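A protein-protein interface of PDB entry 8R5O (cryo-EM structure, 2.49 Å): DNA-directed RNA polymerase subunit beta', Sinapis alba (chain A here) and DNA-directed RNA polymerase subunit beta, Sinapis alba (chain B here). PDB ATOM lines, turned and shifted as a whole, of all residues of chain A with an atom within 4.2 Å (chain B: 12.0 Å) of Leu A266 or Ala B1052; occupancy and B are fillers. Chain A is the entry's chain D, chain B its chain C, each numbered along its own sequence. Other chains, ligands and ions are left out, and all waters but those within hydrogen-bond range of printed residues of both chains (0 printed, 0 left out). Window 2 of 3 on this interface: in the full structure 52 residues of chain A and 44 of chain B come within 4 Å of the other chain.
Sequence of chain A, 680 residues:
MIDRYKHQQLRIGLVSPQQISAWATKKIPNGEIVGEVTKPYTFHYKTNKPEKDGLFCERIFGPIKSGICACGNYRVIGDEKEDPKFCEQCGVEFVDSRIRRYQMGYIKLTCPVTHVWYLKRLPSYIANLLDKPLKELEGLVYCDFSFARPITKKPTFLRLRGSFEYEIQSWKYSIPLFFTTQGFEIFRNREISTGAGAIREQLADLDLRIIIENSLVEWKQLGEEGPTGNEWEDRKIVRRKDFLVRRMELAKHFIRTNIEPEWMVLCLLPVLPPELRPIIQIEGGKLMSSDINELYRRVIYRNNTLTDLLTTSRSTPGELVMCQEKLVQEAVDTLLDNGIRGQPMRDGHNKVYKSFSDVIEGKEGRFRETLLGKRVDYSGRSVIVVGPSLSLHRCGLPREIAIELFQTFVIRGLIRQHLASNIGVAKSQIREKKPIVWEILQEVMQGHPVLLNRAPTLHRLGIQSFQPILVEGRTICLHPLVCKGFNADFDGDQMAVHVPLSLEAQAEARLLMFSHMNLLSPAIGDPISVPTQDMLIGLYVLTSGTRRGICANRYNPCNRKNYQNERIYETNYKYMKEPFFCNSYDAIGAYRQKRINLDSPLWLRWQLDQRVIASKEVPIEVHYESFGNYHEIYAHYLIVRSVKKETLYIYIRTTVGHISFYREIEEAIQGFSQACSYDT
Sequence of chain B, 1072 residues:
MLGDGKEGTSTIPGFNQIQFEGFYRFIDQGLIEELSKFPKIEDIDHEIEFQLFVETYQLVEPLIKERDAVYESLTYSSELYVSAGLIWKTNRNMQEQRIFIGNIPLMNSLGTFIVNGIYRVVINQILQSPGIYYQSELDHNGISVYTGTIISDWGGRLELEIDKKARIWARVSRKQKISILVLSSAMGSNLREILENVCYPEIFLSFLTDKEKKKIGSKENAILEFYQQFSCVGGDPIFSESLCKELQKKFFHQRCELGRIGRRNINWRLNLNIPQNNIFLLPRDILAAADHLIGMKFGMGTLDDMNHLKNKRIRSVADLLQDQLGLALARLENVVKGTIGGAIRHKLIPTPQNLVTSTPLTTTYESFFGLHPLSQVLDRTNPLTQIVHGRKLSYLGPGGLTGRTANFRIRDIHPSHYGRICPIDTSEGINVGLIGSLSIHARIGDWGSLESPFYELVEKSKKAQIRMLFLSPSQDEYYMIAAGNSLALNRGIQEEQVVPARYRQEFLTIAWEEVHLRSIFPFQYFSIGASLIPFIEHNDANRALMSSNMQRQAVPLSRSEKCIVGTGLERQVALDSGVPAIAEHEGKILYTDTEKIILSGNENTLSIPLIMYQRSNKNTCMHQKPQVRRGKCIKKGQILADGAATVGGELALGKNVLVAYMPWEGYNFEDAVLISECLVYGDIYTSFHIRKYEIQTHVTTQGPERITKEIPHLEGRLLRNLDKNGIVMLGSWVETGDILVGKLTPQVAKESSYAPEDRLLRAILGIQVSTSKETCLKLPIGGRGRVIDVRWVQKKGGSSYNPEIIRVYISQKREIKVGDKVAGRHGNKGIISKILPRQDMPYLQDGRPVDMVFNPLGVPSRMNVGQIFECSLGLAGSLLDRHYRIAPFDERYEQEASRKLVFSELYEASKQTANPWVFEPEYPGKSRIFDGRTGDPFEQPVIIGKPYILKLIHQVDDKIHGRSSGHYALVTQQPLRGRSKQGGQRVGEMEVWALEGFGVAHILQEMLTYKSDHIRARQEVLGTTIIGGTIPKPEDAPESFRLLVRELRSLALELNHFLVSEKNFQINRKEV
The backbone carbonyl oxygen (O) of Leu B1051 lies within hydrogen-bond range of a ring nitrogen (NE2) of His A115 (3.2 Å).
The backbone carbonyl oxygen (O) of Ala B1052 sits at hydrogen-bond distance from the backbone NH (N) of Val A15 (3.2 Å).
The backbone NH (N) of Glu B1054 is in hydrogen-bond range of the backbone carbonyl oxygen (O) of Gly A13 (3.3 Å).
The backbone carbonyl oxygen (O) of Leu B1048 lies within hydrogen-bond range of the backbone NH (N) of Leu B1053 (3.2 Å).
The side-chain amide nitrogen (ND2) of Asn B1056 lies within hydrogen-bond range of the side-chain carboxylate (OE1) of Glu B1054 (3.1 Å).
The backbone NH (N) of Leu A266 sits at hydrogen-bond distance from the backbone carbonyl oxygen (O) of Val A113 (2.6 Å).
O of Met A264 lies within hydrogen-bond range of N of His A115.
Leu B1053 touches Gly A13.
Leu A14 touches Ala B1052 (CD2 to O, 3.4 Å).
Leu B1053 touches Val A15.
N of Glu B1054 touches CG2 of Val A15, at 3.4 Å.
Ala B1052 touches Leu A266 (CB to CD2, 3.8 Å).
CD2 of Leu A336 touches O of Ser B1050 (3.8 Å).
Leu A336 touches Leu B1051.
Printed residues of chain B within 4 Å of Gly A13: Leu B1053 and Glu B1054.
Of chain B, only Ala B1052 comes within 4 Å of Leu A14.
No residue of chain B comes within 4 Å of Val A113.
Of chain B, only Leu B1051 (3.2 Å) comes within 4 Å of His A115.
No residue of chain B comes within 4 Å of Val A265.
Leu A266 touches just one residue of chain B: Ala B1052.
Cys A267 touches none of the printed residues of chain B.
No residue of chain B comes within 4 Å of Leu A268.
Of the printed residues of chain B, Leu A336 touches Ser B1050 (3.8 Å) and Leu B1051 (3.8 Å).
Leu B1048 touches none of the printed residues of chain A.
Of the printed residues of chain A, Ser B1050 touches Leu A336.
Printed residues of chain A within 4 Å of Leu B1051: His A115 and Leu A336.
Of chain A, only Leu A14 (3.4 Å), Val A15 (3.2 Å) and Leu A266 (3.8 Å) come within 4 Å of Ala B1052.
Of the printed residues of chain A, Leu B1053 touches Gly A13 (3.6 Å) and Val A15 (3.6 Å).
Of the printed residues of chain A, Glu B1054 touches Gly A13 (3.3 Å) and Val A15 (3.4 Å).
The nearest residue of chain B that does not touch Leu A266 is Leu B1051 (5.9 Å).
Of the 14 printed residues of chain B, 5 touch a printed residue of chain A.
Printed residues of chain B that touch a printed residue of chain A: Ser B1050, Leu B1051, Ala B1052, Leu B1053 and Glu B1054.
Hydrophobic or aromatic side chains of chain B within 4 Å of the printed part of chain A: Leu B1051 and Ala B1052.
Along chain B the printed residues that touch a printed residue of chain A span positions 1050 to 1054.
Printed residues of chain A that touch a printed residue of chain B: Gly A13, Leu A14, Val A15, His A115, Leu A266 and Leu A336.
Among the printed residues, no Asp or Glu carboxylate lies within 4 Å of a Lys or Arg side-chain nitrogen of the other chain.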
ATOM      1  N   GLY A  13      15.174  19.240 -23.715  1.00  0.00           N
ATOM      2  CA  GLY A  13      15.627  20.283 -22.819  1.00  0.00           C
ATOM      3  C   GLY A  13      17.135  20.263 -22.732  1.00  0.00           C
ATOM      4  O   GLY A  13      17.779  19.243 -22.995  1.00  0.00           O
ATOM      5  N   LEU A  14      17.696  21.414 -22.373  1.00  0.00           N
ATOM      6  CA  LEU A  14      19.120  21.478 -22.087  1.00  0.00           C
ATOM      7  C   LEU A  14      19.437  20.603 -20.881  1.00  0.00           C
ATOM      8  O   LEU A  14      18.630  20.460 -19.959  1.00  0.00           O
ATOM      9  CB  LEU A  14      19.556  22.920 -21.832  1.00  0.00           C
ATOM     10  CG  LEU A  14      20.543  23.512 -22.837  1.00  0.00           C
ATOM     11  CD1 LEU A  14      20.922  24.924 -22.428  1.00  0.00           C
ATOM     12  CD2 LEU A  14      21.780  22.635 -22.960  1.00  0.00           C
ATOM     13  N   VAL A  15      20.625  20.012 -20.894  1.00  0.00           N
ATOM     14  CA  VAL A  15      20.992  18.953 -19.964  1.00  0.00           C
ATOM     15  C   VAL A  15      21.976  19.496 -18.940  1.00  0.00           C
ATOM     16  O   VAL A  15      22.953  20.168 -19.292  1.00  0.00           O
ATOM     17  CB  VAL A  15      21.580  17.747 -20.717  1.00  0.00           C
ATOM     18  CG1 VAL A  15      22.066  16.697 -19.745  1.00  0.00           C
ATOM     19  CG2 VAL A  15      20.537  17.168 -21.653  1.00  0.00           C
ATOM     20  N   LEU A 109      35.857  18.515 -18.622  1.00  0.00           N
ATOM     21  CA  LEU A 109      36.609  19.671 -19.089  1.00  0.00           C
ATOM     22  C   LEU A 109      37.271  20.386 -17.919  1.00  0.00           C
ATOM     23  O   LEU A 109      36.627  20.674 -16.905  1.00  0.00           O
ATOM     24  CB  LEU A 109      35.690  20.631 -19.837  1.00  0.00           C
ATOM     25  CG  LEU A 109      35.018  20.106 -21.106  1.00  0.00           C
ATOM     26  CD1 LEU A 109      34.036  21.128 -21.647  1.00  0.00           C
ATOM     27  CD2 LEU A 109      36.058  19.754 -22.153  1.00  0.00           C
ATOM     28  N   PRO A 112      35.395  25.381 -18.378  1.00  0.00           N
ATOM     29  CA  PRO A 112      34.091  25.377 -19.048  1.00  0.00           C
ATOM     30  C   PRO A 112      34.155  26.054 -20.407  1.00  0.00           C
ATOM     31  O   PRO A 112      34.937  26.982 -20.631  1.00  0.00           O
ATOM     32  CB  PRO A 112      33.191  26.155 -18.081  1.00  0.00           C
ATOM     33  CG  PRO A 112      34.129  26.978 -17.265  1.00  0.00           C
ATOM     34  CD  PRO A 112      35.383  26.171 -17.136  1.00  0.00           C
ATOM     35  N   VAL A 113      33.320  25.572 -21.325  1.00  0.00           N
ATOM     36  CA  VAL A 113      33.235  26.111 -22.677  1.00  0.00           C
ATOM     37  C   VAL A 113      31.776  26.401 -23.001  1.00  0.00           C
ATOM     38  O   VAL A 113      30.878  25.657 -22.592  1.00  0.00           O
ATOM     39  CB  VAL A 113      33.849  25.151 -23.722  1.00  0.00           C
ATOM     40  CG1 VAL A 113      35.301  24.854 -23.387  1.00  0.00           C
ATOM     41  CG2 VAL A 113      33.047  23.866 -23.818  1.00  0.00           C
ATOM     42  N   HIS A 115      28.422  26.618 -25.258  1.00  0.00           N
ATOM     43  CA  HIS A 115      27.808  25.852 -26.334  1.00  0.00           C
ATOM     44  C   HIS A 115      27.646  26.767 -27.542  1.00  0.00           C
ATOM     45  O   HIS A 115      27.034  27.835 -27.440  1.00  0.00           O
ATOM     46  CB  HIS A 115      26.463  25.286 -25.885  1.00  0.00           C
ATOM     47  CG  HIS A 115      25.942  24.187 -26.758  1.00  0.00           C
ATOM     48  ND1 HIS A 115      25.757  24.334 -28.115  1.00  0.00           N
ATOM     49  CD2 HIS A 115      25.548  22.927 -26.459  1.00  0.00           C
ATOM     50  CE1 HIS A 115      25.281  23.210 -28.616  1.00  0.00           C
ATOM     51  NE2 HIS A 115      25.144  22.340 -27.633  1.00  0.00           N
ATOM     52  N   MET A 264      23.894  26.565 -20.621  1.00  0.00           N
ATOM     53  CA  MET A 264      24.399  26.940 -21.934  1.00  0.00           C
ATOM     54  C   MET A 264      25.922  26.962 -21.987  1.00  0.00           C
ATOM     55  O   MET A 264      26.485  26.991 -23.086  1.00  0.00           O
ATOM     56  CB  MET A 264      23.833  28.302 -22.343  1.00  0.00           C
ATOM     57  CG  MET A 264      22.322  28.300 -22.539  1.00  0.00           C
ATOM     58  SD  MET A 264      21.661  29.808 -23.274  1.00  0.00           S
ATOM     59  CE  MET A 264      21.870  30.973 -21.935  1.00  0.00           C
ATOM     60  N   VAL A 265      26.595  26.943 -20.839  1.00  0.00           N
ATOM     61  CA  VAL A 265      28.044  26.805 -20.766  1.00  0.00           C
ATOM     62  C   VAL A 265      28.342  25.395 -20.276  1.00  0.00           C
ATOM     63  O   VAL A 265      27.922  25.010 -19.179  1.00  0.00           O
ATOM     64  CB  VAL A 265      28.674  27.858 -19.842  1.00  0.00           C
ATOM     65  CG1 VAL A 265      30.191  27.754 -19.874  1.00  0.00           C
ATOM     66  CG2 VAL A 265      28.221  29.253 -20.239  1.00  0.00           C
ATOM     67  N   LEU A 266      29.064  24.629 -21.086  1.00  0.00           N
ATOM     68  CA  LEU A 266      29.294  23.220 -20.799  1.00  0.00           C
ATOM     69  C   LEU A 266      30.457  23.041 -19.833  1.00  0.00           C
ATOM     70  O   LEU A 266      31.553  23.560 -20.061  1.00  0.00           O
ATOM     71  CB  LEU A 266      29.568  22.455 -22.092  1.00  0.00           C
ATOM     72  CG  LEU A 266      28.419  22.361 -23.096  1.00  0.00           C
ATOM     73  CD1 LEU A 266      28.893  21.722 -24.388  1.00  0.00           C
ATOM     74  CD2 LEU A 266      27.264  21.575 -22.503  1.00  0.00           C
ATOM     75  N   CYS A 267      30.212  22.304 -18.751  1.00  0.00           N
ATOM     76  CA  CYS A 267      31.272  21.858 -17.857  1.00  0.00           C
ATOM     77  C   CYS A 267      31.736  20.443 -18.163  1.00  0.00           C
ATOM     78  O   CYS A 267      32.919  20.138 -17.990  1.00  0.00           O
ATOM     79  CB  CYS A 267      30.807  21.933 -16.400  1.00  0.00           C
ATOM     80  SG  CYS A 267      30.376  23.596 -15.849  1.00  0.00           S
ATOM     81  N   LEU A 268      30.830  19.579 -18.610  1.00  0.00           N
ATOM     82  CA  LEU A 268      31.157  18.234 -19.052  1.00  0.00           C
ATOM     83  C   LEU A 268      30.739  18.071 -20.506  1.00  0.00           C
ATOM     84  O   LEU A 268      29.820  18.741 -20.983  1.00  0.00           O
ATOM     85  CB  LEU A 268      30.463  17.178 -18.190  1.00  0.00           C
ATOM     86  CG  LEU A 268      30.720  17.267 -16.686  1.00  0.00           C
ATOM     87  CD1 LEU A 268      29.878  16.247 -15.955  1.00  0.00           C
ATOM     88  CD2 LEU A 268      32.195  17.068 -16.383  1.00  0.00           C
ATOM     89  N   LEU A 336      30.936  20.414 -32.013  1.00  0.00           N
ATOM     90  CA  LEU A 336      29.490  20.597 -31.917  1.00  0.00           C
ATOM     91  C   LEU A 336      28.899  21.128 -33.217  1.00  0.00           C
ATOM     92  O   LEU A 336      27.956  20.542 -33.760  1.00  0.00           O
ATOM     93  CB  LEU A 336      29.151  21.531 -30.754  1.00  0.00           C
ATOM     94  CG  LEU A 336      29.445  21.011 -29.345  1.00  0.00           C
ATOM     95  CD1 LEU A 336      28.913  21.974 -28.292  1.00  0.00           C
ATOM     96  CD2 LEU A 336      28.864  19.622 -29.148  1.00  0.00           C
ATOM     97  N   LEU B1043      18.774   5.534 -31.839  1.00  0.00           N
ATOM     98  CA  LEU B1043      20.016   6.131 -32.314  1.00  0.00           C
ATOM     99  C   LEU B1043      19.913   7.647 -32.398  1.00  0.00           C
ATOM    100  O   LEU B1043      20.913   8.345 -32.205  1.00  0.00           O
ATOM    101  CB  LEU B1043      20.396   5.544 -33.673  1.00  0.00           C
ATOM    102  CG  LEU B1043      21.294   4.303 -33.695  1.00  0.00           C
ATOM    103  CD1 LEU B1043      20.741   3.179 -32.831  1.00  0.00           C
ATOM    104  CD2 LEU B1043      21.499   3.824 -35.124  1.00  0.00           C
ATOM    105  N   LEU B1044      18.720   8.173 -32.689  1.00  0.00           N
ATOM    106  CA  LEU B1044      18.531   9.620 -32.723  1.00  0.00           C
ATOM    107  C   LEU B1044      18.738  10.242 -31.347  1.00  0.00           C
ATOM    108  O   LEU B1044      19.311  11.331 -31.232  1.00  0.00           O
ATOM    109  CB  LEU B1044      17.136   9.955 -33.251  1.00  0.00           C
ATOM    110  CG  LEU B1044      16.674  11.406 -33.099  1.00  0.00           C
ATOM    111  CD1 LEU B1044      17.517  12.335 -33.956  1.00  0.00           C
ATOM    112  CD2 LEU B1044      15.200  11.541 -33.439  1.00  0.00           C
ATOM    113  N   VAL B1045      18.270   9.567 -30.295  1.00  0.00           N
ATOM    114  CA  VAL B1045      18.391  10.107 -28.944  1.00  0.00           C
ATOM    115  C   VAL B1045      19.855  10.253 -28.552  1.00  0.00           C
ATOM    116  O   VAL B1045      20.255  11.259 -27.956  1.00  0.00           O
ATOM    117  CB  VAL B1045      17.623   9.221 -27.947  1.00  0.00           C
ATOM    118  CG1 VAL B1045      17.824   9.718 -26.526  1.00  0.00           C
ATOM    119  CG2 VAL B1045      16.148   9.185 -28.299  1.00  0.00           C
ATOM    120  N   ARG B1046      20.678   9.253 -28.879  1.00  0.00           N
ATOM    121  CA  ARG B1046      22.088   9.304 -28.509  1.00  0.00           C
ATOM    122  C   ARG B1046      22.815  10.431 -29.229  1.00  0.00           C
ATOM    123  O   ARG B1046      23.669  11.102 -28.639  1.00  0.00           O
ATOM    124  CB  ARG B1046      22.759   7.962 -28.800  1.00  0.00           C
ATOM    125  CG  ARG B1046      22.198   6.801 -28.000  1.00  0.00           C
ATOM    126  CD  ARG B1046      22.071   7.162 -26.533  1.00  0.00           C
ATOM    127  NE  ARG B1046      21.702   6.014 -25.712  1.00  0.00           N
ATOM    128  CZ  ARG B1046      20.465   5.560 -25.571  1.00  0.00           C
ATOM    129  NH1 ARG B1046      19.446   6.115 -26.205  1.00  0.00           N
ATOM    130  NH2 ARG B1046      20.243   4.521 -24.771  1.00  0.00           N
ATOM    131  N   GLU B1047      22.499  10.653 -30.507  1.00  0.00           N
ATOM    132  CA  GLU B1047      23.134  11.744 -31.237  1.00  0.00           C
ATOM    133  C   GLU B1047      22.717  13.103 -30.689  1.00  0.00           C
ATOM    134  O   GLU B1047      23.526  14.038 -30.677  1.00  0.00           O
ATOM    135  CB  GLU B1047      22.809  11.641 -32.725  1.00  0.00           C
ATOM    136  CG  GLU B1047      23.096  10.269 -33.311  1.00  0.00           C
ATOM    137  CD  GLU B1047      23.801  10.332 -34.649  1.00  0.00           C
ATOM    138  OE1 GLU B1047      24.590  11.277 -34.860  1.00  0.00           O
ATOM    139  OE2 GLU B1047      23.569   9.435 -35.487  1.00  0.00           O
ATOM    140  N   LEU B1048      21.467  13.237 -30.240  1.00  0.00           N
ATOM    141  CA  LEU B1048      21.053  14.464 -29.571  1.00  0.00           C
ATOM    142  C   LEU B1048      21.730  14.615 -28.216  1.00  0.00           C
ATOM    143  O   LEU B1048      21.998  15.741 -27.782  1.00  0.00           O
ATOM    144  CB  LEU B1048      19.534  14.498 -29.410  1.00  0.00           C
ATOM    145  CG  LEU B1048      18.719  14.664 -30.692  1.00  0.00           C
ATOM    146  CD1 LEU B1048      17.234  14.717 -30.381  1.00  0.00           C
ATOM    147  CD2 LEU B1048      19.159  15.914 -31.433  1.00  0.00           C
ATOM    148  N   ARG B1049      22.009  13.500 -27.536  1.00  0.00           N
ATOM    149  CA  ARG B1049      22.723  13.567 -26.266  1.00  0.00           C
ATOM    150  C   ARG B1049      24.137  14.095 -26.447  1.00  0.00           C
ATOM    151  O   ARG B1049      24.691  14.706 -25.528  1.00  0.00           O
ATOM    152  CB  ARG B1049      22.759  12.192 -25.603  1.00  0.00           C
ATOM    153  CG  ARG B1049      21.442  11.759 -25.012  1.00  0.00           C
ATOM    154  CD  ARG B1049      21.591  10.469 -24.247  1.00  0.00           C
ATOM    155  NE  ARG B1049      20.331  10.053 -23.647  1.00  0.00           N
ATOM    156  CZ  ARG B1049      20.191   8.999 -22.856  1.00  0.00           C
ATOM    157  NH1 ARG B1049      21.221   8.232 -22.539  1.00  0.00           N
ATOM    158  NH2 ARG B1049      18.989   8.710 -22.367  1.00  0.00           N
ATOM    159  N   SER B1050      24.738  13.868 -27.616  1.00  0.00           N
ATOM    160  CA  SER B1050      26.064  14.402 -27.893  1.00  0.00           C
ATOM    161  C   SER B1050      26.070  15.924 -27.964  1.00  0.00           C
ATOM    162  O   SER B1050      27.140  16.533 -27.872  1.00  0.00           O
ATOM    163  CB  SER B1050      26.599  13.816 -29.199  1.00  0.00           C
ATOM    164  OG  SER B1050      25.769  14.167 -30.290  1.00  0.00           O
ATOM    165  N   LEU B1051      24.903  16.548 -28.124  1.00  0.00           N
ATOM    166  CA  LEU B1051      24.773  17.998 -28.146  1.00  0.00           C
ATOM    167  C   LEU B1051      24.190  18.542 -26.847  1.00  0.00           C
ATOM    168  O   LEU B1051      23.668  19.660 -26.827  1.00  0.00           O
ATOM    169  CB  LEU B1051      23.921  18.429 -29.338  1.00  0.00           C
ATOM    170  CG  LEU B1051      24.529  18.176 -30.719  1.00  0.00           C
ATOM    171  CD1 LEU B1051      23.440  17.998 -31.759  1.00  0.00           C
ATOM    172  CD2 LEU B1051      25.455  19.318 -31.109  1.00  0.00           C
ATOM    173  N   ALA B1052      24.270  17.761 -25.766  1.00  0.00           N
ATOM    174  CA  ALA B1052      23.746  18.142 -24.452  1.00  0.00           C
ATOM    175  C   ALA B1052      22.242  18.414 -24.499  1.00  0.00           C
ATOM    176  O   ALA B1052      21.738  19.336 -23.856  1.00  0.00           O
ATOM    177  CB  ALA B1052      24.500  19.343 -23.877  1.00  0.00           C
ATOM    178  N   LEU B1053      21.521  17.603 -25.266  1.00  0.00           N
ATOM    179  CA  LEU B1053      20.066  17.641 -25.312  1.00  0.00           C
ATOM    180  C   LEU B1053      19.523  16.267 -24.956  1.00  0.00           C
ATOM    181  O   LEU B1053      20.043  15.249 -25.417  1.00  0.00           O
ATOM    182  CB  LEU B1053      19.556  18.052 -26.695  1.00  0.00           C
ATOM    183  CG  LEU B1053      20.184  19.271 -27.368  1.00  0.00           C
ATOM    184  CD1 LEU B1053      19.515  19.533 -28.704  1.00  0.00           C
ATOM    185  CD2 LEU B1053      20.100  20.493 -26.474  1.00  0.00           C
ATOM    186  N   GLU B1054      18.478  16.237 -24.138  1.00  0.00           N
ATOM    187  CA  GLU B1054      17.807  14.994 -23.790  1.00  0.00           C
ATOM    188  C   GLU B1054      16.397  14.995 -24.362  1.00  0.00           C
ATOM    189  O   GLU B1054      15.685  15.999 -24.287  1.00  0.00           O
ATOM    190  CB  GLU B1054      17.766  14.779 -22.273  1.00  0.00           C
ATOM    191  CG  GLU B1054      17.014  15.834 -21.489  1.00  0.00           C
ATOM    192  CD  GLU B1054      16.708  15.380 -20.079  1.00  0.00           C
ATOM    193  OE1 GLU B1054      16.859  14.171 -19.803  1.00  0.00           O
ATOM    194  OE2 GLU B1054      16.316  16.225 -19.248  1.00  0.00           O
ATOM    195  N   LEU B1055      16.007  13.866 -24.942  1.00  0.00           N
ATOM    196  CA  LEU B1055      14.702  13.696 -25.575  1.00  0.00           C
ATOM    197  C   LEU B1055      13.996  12.536 -24.879  1.00  0.00           C
ATOM    198  O   LEU B1055      14.265  11.369 -25.178  1.00  0.00           O
ATOM    199  CB  LEU B1055      14.864  13.453 -27.073  1.00  0.00           C
ATOM    200  CG  LEU B1055      13.624  13.194 -27.926  1.00  0.00           C
ATOM    201  CD1 LEU B1055      12.646  14.348 -27.818  1.00  0.00           C
ATOM    202  CD2 LEU B1055      14.028  12.969 -29.371  1.00  0.00           C
ATOM    203  N   ASN B1056      13.090  12.856 -23.961  1.00  0.00           N
ATOM    204  CA  ASN B1056      12.393  11.856 -23.165  1.00  0.00           C
ATOM    205  C   ASN B1056      10.982  11.648 -23.692  1.00  0.00           C
ATOM    206  O   ASN B1056      10.292  12.608 -24.039  1.00  0.00           O
ATOM    207  CB  ASN B1056      12.334  12.271 -21.694  1.00  0.00           C
ATOM    208  CG  ASN B1056      13.692  12.611 -21.131  1.00  0.00           C
ATOM    209  OD1 ASN B1056      14.485  11.726 -20.816  1.00  0.00           O
ATOM    210  ND2 ASN B1056      13.968  13.901 -20.991  1.00  0.00           N
